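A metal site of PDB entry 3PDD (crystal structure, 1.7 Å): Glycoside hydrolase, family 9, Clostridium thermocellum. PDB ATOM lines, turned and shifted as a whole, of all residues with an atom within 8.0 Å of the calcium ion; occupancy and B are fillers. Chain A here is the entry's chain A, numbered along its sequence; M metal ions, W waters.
OD1 of Asp 163 sits at hydrogen-bond distance from N of Asp 165, 2.8 Å away. The backbone NH (N) of Ala 167 is in hydrogen-bond range of the side-chain carboxylate (OD1) of Asp 163 (2.9 Å). N of Asp 166 sits at hydrogen-bond distance from OD1 of Asp 163, 3.0 Å away. The side-chain carboxylate (OD2) of Asp 119 lies close to the backbone NH (N) of Gly 122 (2.9 Å). The side-chain carboxylate (OD2) of Asp 119 sits close to the backbone NH (N) of Lys 123. The side-chain carboxylate (OD2) of Asp 121 lies within salt-bridge range of the side-chain amino group (NZ) of Lys 87, at 3.7 Å.
The calcium ion is bound by O of Val 90, OD2 of Asp 163, OD2 of Asp 119, OD1 of Asp 121, OD1 of Asp 119, water W2 and water W1. The calcium ion has seven donor atoms within binding distance.
Water W2 lies within hydrogen-bond range of OD1 of Asp 164 (2.6 Å) and OD2 of Asp 165 (2.8 Å). Water W1 lies within hydrogen-bond range of OD2 of Asp 121 (2.5 Å), OD2 of Asp 165 (2.6 Å) and N of Val 90 (3.0 Å).
Along chain A the residues within 4 Å of the calcium ion span positions 90 to 163.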
ATOM      1  N   LYS A  87       2.101  -1.431  -8.481  1.00  0.00           N
ATOM      2  CA  LYS A  87       1.714  -2.672  -7.772  1.00  0.00           C
ATOM      3  C   LYS A  87       0.717  -3.501  -8.576  1.00  0.00           C
ATOM      4  O   LYS A  87       0.148  -3.013  -9.550  1.00  0.00           O
ATOM      5  CB  LYS A  87       1.177  -2.344  -6.390  1.00  0.00           C
ATOM      6  CG  LYS A  87      -0.173  -1.566  -6.374  1.00  0.00           C
ATOM      7  CD  LYS A  87      -0.634  -1.148  -5.029  1.00  0.00           C
ATOM      8  CE  LYS A  87      -1.105  -2.377  -4.278  1.00  0.00           C
ATOM      9  NZ  LYS A  87      -1.756  -2.014  -2.998  1.00  0.00           N
ATOM     10  N   VAL A  88       0.529  -4.763  -8.145  1.00  0.00           N
ATOM     11  CA  VAL A  88      -0.544  -5.602  -8.589  1.00  0.00           C
ATOM     12  C   VAL A  88      -1.794  -5.025  -7.896  1.00  0.00           C
ATOM     13  O   VAL A  88      -1.847  -4.880  -6.662  1.00  0.00           O
ATOM     14  CB  VAL A  88      -0.289  -7.061  -8.214  1.00  0.00           C
ATOM     15  CG1 VAL A  88      -1.552  -7.895  -8.378  1.00  0.00           C
ATOM     16  CG2 VAL A  88       0.894  -7.663  -9.057  1.00  0.00           C
ATOM     17  N   ILE A  89      -2.812  -4.707  -8.694  1.00  0.00           N
ATOM     18  CA  ILE A  89      -4.013  -4.118  -8.135  1.00  0.00           C
ATOM     19  C   ILE A  89      -5.011  -5.252  -8.041  1.00  0.00           C
ATOM     20  O   ILE A  89      -5.149  -6.067  -8.991  1.00  0.00           O
ATOM     21  CB  ILE A  89      -4.532  -2.953  -9.053  1.00  0.00           C
ATOM     22  CG1 ILE A  89      -3.518  -1.784  -9.122  1.00  0.00           C
ATOM     23  CG2 ILE A  89      -5.925  -2.480  -8.565  1.00  0.00           C
ATOM     24  CD1 ILE A  89      -3.368  -0.926  -7.826  1.00  0.00           C
ATOM     25  N   VAL A  90      -5.714  -5.321  -6.922  1.00  0.00           N
ATOM     26  CA  VAL A  90      -6.684  -6.389  -6.651  1.00  0.00           C
ATOM     27  C   VAL A  90      -7.926  -5.683  -6.088  1.00  0.00           C
ATOM     28  O   VAL A  90      -7.890  -5.066  -4.997  1.00  0.00           O
ATOM     29  CB  VAL A  90      -6.181  -7.405  -5.609  1.00  0.00           C
ATOM     30  CG1 VAL A  90      -7.260  -8.546  -5.466  1.00  0.00           C
ATOM     31  CG2 VAL A  90      -4.803  -8.003  -5.990  1.00  0.00           C
ATOM     32  N   LYS A  91      -9.014  -5.713  -6.865  1.00  0.00           N
ATOM     33  CA  LYS A  91     -10.190  -4.934  -6.499  1.00  0.00           C
ATOM     34  C   LYS A  91     -10.804  -5.592  -5.245  1.00  0.00           C
ATOM     35  O   LYS A  91     -10.626  -6.811  -5.018  1.00  0.00           O
ATOM     36  CB  LYS A  91     -11.193  -4.774  -7.666  1.00  0.00           C
ATOM     37  CG  LYS A  91     -11.938  -6.011  -8.091  1.00  0.00           C
ATOM     38  CD  LYS A  91     -12.930  -5.754  -9.287  1.00  0.00           C
ATOM     39  CE  LYS A  91     -12.254  -5.239 -10.570  1.00  0.00           C
ATOM     40  NZ  LYS A  91     -11.527  -6.302 -11.342  1.00  0.00           N
ATOM     41  N   PRO A  92     -11.433  -4.742  -4.400  1.00  0.00           N
ATOM     42  CA  PRO A  92     -12.142  -5.252  -3.188  1.00  0.00           C
ATOM     43  C   PRO A  92     -13.399  -5.985  -3.591  1.00  0.00           C
ATOM     44  O   PRO A  92     -13.766  -6.049  -4.762  1.00  0.00           O
ATOM     45  CB  PRO A  92     -12.492  -3.968  -2.413  1.00  0.00           C
ATOM     46  CG  PRO A  92     -12.587  -2.861  -3.407  1.00  0.00           C
ATOM     47  CD  PRO A  92     -11.583  -3.254  -4.511  1.00  0.00           C
ATOM     48  N   THR A  93     -14.067  -6.585  -2.621  1.00  0.00           N
ATOM     49  CA  THR A  93     -15.328  -7.252  -2.867  1.00  0.00           C
ATOM     50  C   THR A  93     -16.318  -6.635  -1.829  1.00  0.00           C
ATOM     51  O   THR A  93     -15.917  -6.087  -0.824  1.00  0.00           O
ATOM     52  CB  THR A  93     -15.270  -8.800  -2.686  1.00  0.00           C
ATOM     53  OG1 THR A  93     -14.795  -9.093  -1.417  1.00  0.00           O
ATOM     54  CG2 THR A  93     -14.377  -9.473  -3.692  1.00  0.00           C
ATOM     55  N   SER A 118     -14.562  -6.413   1.796  1.00  0.00           N
ATOM     56  CA  SER A 118     -13.286  -7.092   2.073  1.00  0.00           C
ATOM     57  C   SER A 118     -12.292  -6.720   0.991  1.00  0.00           C
ATOM     58  O   SER A 118     -12.684  -6.574  -0.167  1.00  0.00           O
ATOM     59  CB  SER A 118     -13.500  -8.606   1.992  1.00  0.00           C
ATOM     60  OG  SER A 118     -14.052  -9.153   3.170  1.00  0.00           O
ATOM     61  N   ASP A 119     -11.004  -6.639   1.330  1.00  0.00           N
ATOM     62  CA  ASP A 119      -9.997  -6.406   0.296  1.00  0.00           C
ATOM     63  C   ASP A 119      -8.861  -7.404   0.595  1.00  0.00           C
ATOM     64  O   ASP A 119      -8.334  -7.439   1.698  1.00  0.00           O
ATOM     65  CB  ASP A 119      -9.426  -4.986   0.331  1.00  0.00           C
ATOM     66  CG  ASP A 119      -8.542  -4.711  -0.879  1.00  0.00           C
ATOM     67  OD1 ASP A 119      -8.860  -5.174  -1.984  1.00  0.00           O
ATOM     68  OD2 ASP A 119      -7.555  -4.005  -0.758  1.00  0.00           O
ATOM     69  N   SER A 120      -8.497  -8.199  -0.388  1.00  0.00           N
ATOM     70  CA  SER A 120      -7.558  -9.296  -0.103  1.00  0.00           C
ATOM     71  C   SER A 120      -6.147  -8.821   0.138  1.00  0.00           C
ATOM     72  O   SER A 120      -5.415  -9.455   0.865  1.00  0.00           O
ATOM     73  CB  SER A 120      -7.525 -10.339  -1.239  1.00  0.00           C
ATOM     74  OG  SER A 120      -7.298  -9.741  -2.494  1.00  0.00           O
ATOM     75  N   ASP A 121      -5.754  -7.735  -0.524  1.00  0.00           N
ATOM     76  CA  ASP A 121      -4.405  -7.249  -0.453  1.00  0.00           C
ATOM     77  C   ASP A 121      -4.279  -5.996   0.378  1.00  0.00           C
ATOM     78  O   ASP A 121      -3.196  -5.747   0.877  1.00  0.00           O
ATOM     79  CB  ASP A 121      -3.751  -7.061  -1.865  1.00  0.00           C
ATOM     80  CG  ASP A 121      -4.337  -5.921  -2.658  1.00  0.00           C
ATOM     81  OD1 ASP A 121      -5.544  -5.795  -2.532  1.00  0.00           O
ATOM     82  OD2 ASP A 121      -3.618  -5.151  -3.390  1.00  0.00           O
ATOM     83  N   GLY A 122      -5.340  -5.229   0.572  1.00  0.00           N
ATOM     84  CA  GLY A 122      -5.260  -3.913   1.200  1.00  0.00           C
ATOM     85  C   GLY A 122      -6.390  -3.726   2.226  1.00  0.00           C
ATOM     86  O   GLY A 122      -6.685  -4.592   3.026  1.00  0.00           O
ATOM     87  N   LYS A 123      -6.956  -2.537   2.234  1.00  0.00           N
ATOM     88  CA  LYS A 123      -8.097  -2.272   3.091  1.00  0.00           C
ATOM     89  C   LYS A 123      -9.220  -1.523   2.381  1.00  0.00           C
ATOM     90  O   LYS A 123      -9.055  -1.011   1.302  1.00  0.00           O
ATOM     91  CB  LYS A 123      -7.620  -1.584   4.360  1.00  0.00           C
ATOM     92  CG  LYS A 123      -7.000  -0.242   4.118  1.00  0.00           C
ATOM     93  CD  LYS A 123      -6.210   0.220   5.342  1.00  0.00           C
ATOM     94  CE  LYS A 123      -5.257   1.334   4.960  1.00  0.00           C
ATOM     95  NZ  LYS A 123      -5.938   2.630   4.707  1.00  0.00           N
ATOM     96  N   ILE A 124     -10.393  -1.523   2.998  1.00  0.00           N
ATOM     97  CA  ILE A 124     -11.571  -0.757   2.486  1.00  0.00           C
ATOM     98  C   ILE A 124     -11.492   0.693   2.974  1.00  0.00           C
ATOM     99  O   ILE A 124     -11.346   0.994   4.193  1.00  0.00           O
ATOM    100  CB  ILE A 124     -12.891  -1.401   2.949  1.00  0.00           C
ATOM    101  CG1 ILE A 124     -12.973  -2.851   2.474  1.00  0.00           C
ATOM    102  CG2 ILE A 124     -14.124  -0.570   2.461  1.00  0.00           C
ATOM    103  CD1 ILE A 124     -13.032  -3.003   0.997  1.00  0.00           C
ATOM    104  N   TYR A 162     -14.755   0.551  -2.129  1.00  0.00           N
ATOM    105  CA  TYR A 162     -13.535   1.166  -2.697  1.00  0.00           C
ATOM    106  C   TYR A 162     -12.436   0.858  -1.674  1.00  0.00           C
ATOM    107  O   TYR A 162     -12.627   1.018  -0.483  1.00  0.00           O
ATOM    108  CB  TYR A 162     -13.707   2.680  -2.870  1.00  0.00           C
ATOM    109  CG  TYR A 162     -14.726   2.996  -3.942  1.00  0.00           C
ATOM    110  CD1 TYR A 162     -14.332   3.302  -5.226  1.00  0.00           C
ATOM    111  CD2 TYR A 162     -16.098   2.906  -3.693  1.00  0.00           C
ATOM    112  CE1 TYR A 162     -15.241   3.592  -6.197  1.00  0.00           C
ATOM    113  CE2 TYR A 162     -17.025   3.161  -4.674  1.00  0.00           C
ATOM    114  CZ  TYR A 162     -16.591   3.493  -5.943  1.00  0.00           C
ATOM    115  OH  TYR A 162     -17.488   3.725  -6.969  1.00  0.00           O
ATOM    116  N   ASP A 163     -11.289   0.431  -2.182  1.00  0.00           N
ATOM    117  CA  ASP A 163     -10.120   0.150  -1.362  1.00  0.00           C
ATOM    118  C   ASP A 163      -9.128   1.305  -1.263  1.00  0.00           C
ATOM    119  O   ASP A 163      -9.403   2.422  -1.723  1.00  0.00           O
ATOM    120  CB  ASP A 163      -9.506  -1.167  -1.835  1.00  0.00           C
ATOM    121  CG  ASP A 163      -8.704  -1.047  -3.123  1.00  0.00           C
ATOM    122  OD1 ASP A 163      -8.440   0.064  -3.624  1.00  0.00           O
ATOM    123  OD2 ASP A 163      -8.343  -2.113  -3.648  1.00  0.00           O
ATOM    124  N   ASP A 164      -7.986   1.041  -0.636  1.00  0.00           N
ATOM    125  CA  ASP A 164      -6.959   2.011  -0.404  1.00  0.00           C
ATOM    126  C   ASP A 164      -6.158   2.373  -1.646  1.00  0.00           C
ATOM    127  O   ASP A 164      -5.386   3.311  -1.629  1.00  0.00           O
ATOM    128  CB  ASP A 164      -6.021   1.573   0.748  1.00  0.00           C
ATOM    129  CG  ASP A 164      -5.302   0.219   0.483  1.00  0.00           C
ATOM    130  OD1 ASP A 164      -5.965  -0.740   0.076  1.00  0.00           O
ATOM    131  OD2 ASP A 164      -4.050   0.134   0.711  1.00  0.00           O
ATOM    132  N   ASP A 165      -6.343   1.628  -2.728  1.00  0.00           N
ATOM    133  CA  ASP A 165      -5.819   1.964  -4.038  1.00  0.00           C
ATOM    134  C   ASP A 165      -6.890   2.697  -4.932  1.00  0.00           C
ATOM    135  O   ASP A 165      -6.637   3.003  -6.098  1.00  0.00           O
ATOM    136  CB  ASP A 165      -5.348   0.678  -4.768  1.00  0.00           C
ATOM    137  CG  ASP A 165      -4.141   0.022  -4.101  1.00  0.00           C
ATOM    138  OD1 ASP A 165      -3.263   0.814  -3.636  1.00  0.00           O
ATOM    139  OD2 ASP A 165      -4.061  -1.229  -4.015  1.00  0.00           O
ATOM    140  N   ASP A 166      -8.064   2.950  -4.362  1.00  0.00           N
ATOM    141  CA  ASP A 166      -9.207   3.496  -5.088  1.00  0.00           C
ATOM    142  C   ASP A 166      -9.744   2.599  -6.220  1.00  0.00           C
ATOM    143  O   ASP A 166     -10.415   3.065  -7.163  1.00  0.00           O
ATOM    144  CB  ASP A 166      -8.927   4.888  -5.597  1.00  0.00           C
ATOM    145  CG  ASP A 166     -10.191   5.672  -5.845  1.00  0.00           C
ATOM    146  OD1 ASP A 166     -11.239   5.482  -5.107  1.00  0.00           O
ATOM    147  OD2 ASP A 166     -10.131   6.494  -6.776  1.00  0.00           O
ATOM    148  N   ALA A 167      -9.498   1.294  -6.065  1.00  0.00           N
ATOM    149  CA  ALA A 167     -10.073   0.271  -6.915  1.00  0.00           C
ATOM    150  C   ALA A 167     -11.468  -0.021  -6.393  1.00  0.00           C
ATOM    151  O   ALA A 167     -11.671  -0.150  -5.191  1.00  0.00           O
ATOM    152  CB  ALA A 167      -9.249  -0.989  -6.873  1.00  0.00           C
ATOM    153  N   ALA A 168     -12.422  -0.128  -7.308  1.00  0.00           N
ATOM    154  CA  ALA A 168     -13.790  -0.389  -6.940  1.00  0.00           C
ATOM    155  C   ALA A 168     -14.126  -1.860  -7.110  1.00  0.00           C
ATOM    156  O   ALA A 168     -13.674  -2.532  -8.028  1.00  0.00           O
ATOM    157  CB  ALA A 168     -14.684   0.408  -7.730  1.00  0.00           C
HETATM  158 CA    CA M   1      -7.058  -3.981  -3.112  1.00  0.00          CA
HETATM  159  O   HOH W   1      -5.098  -3.547  -4.637  1.00  0.00           O
HETATM  160  O   HOH W   2      -5.653  -2.327  -1.991  1.00  0.00           O
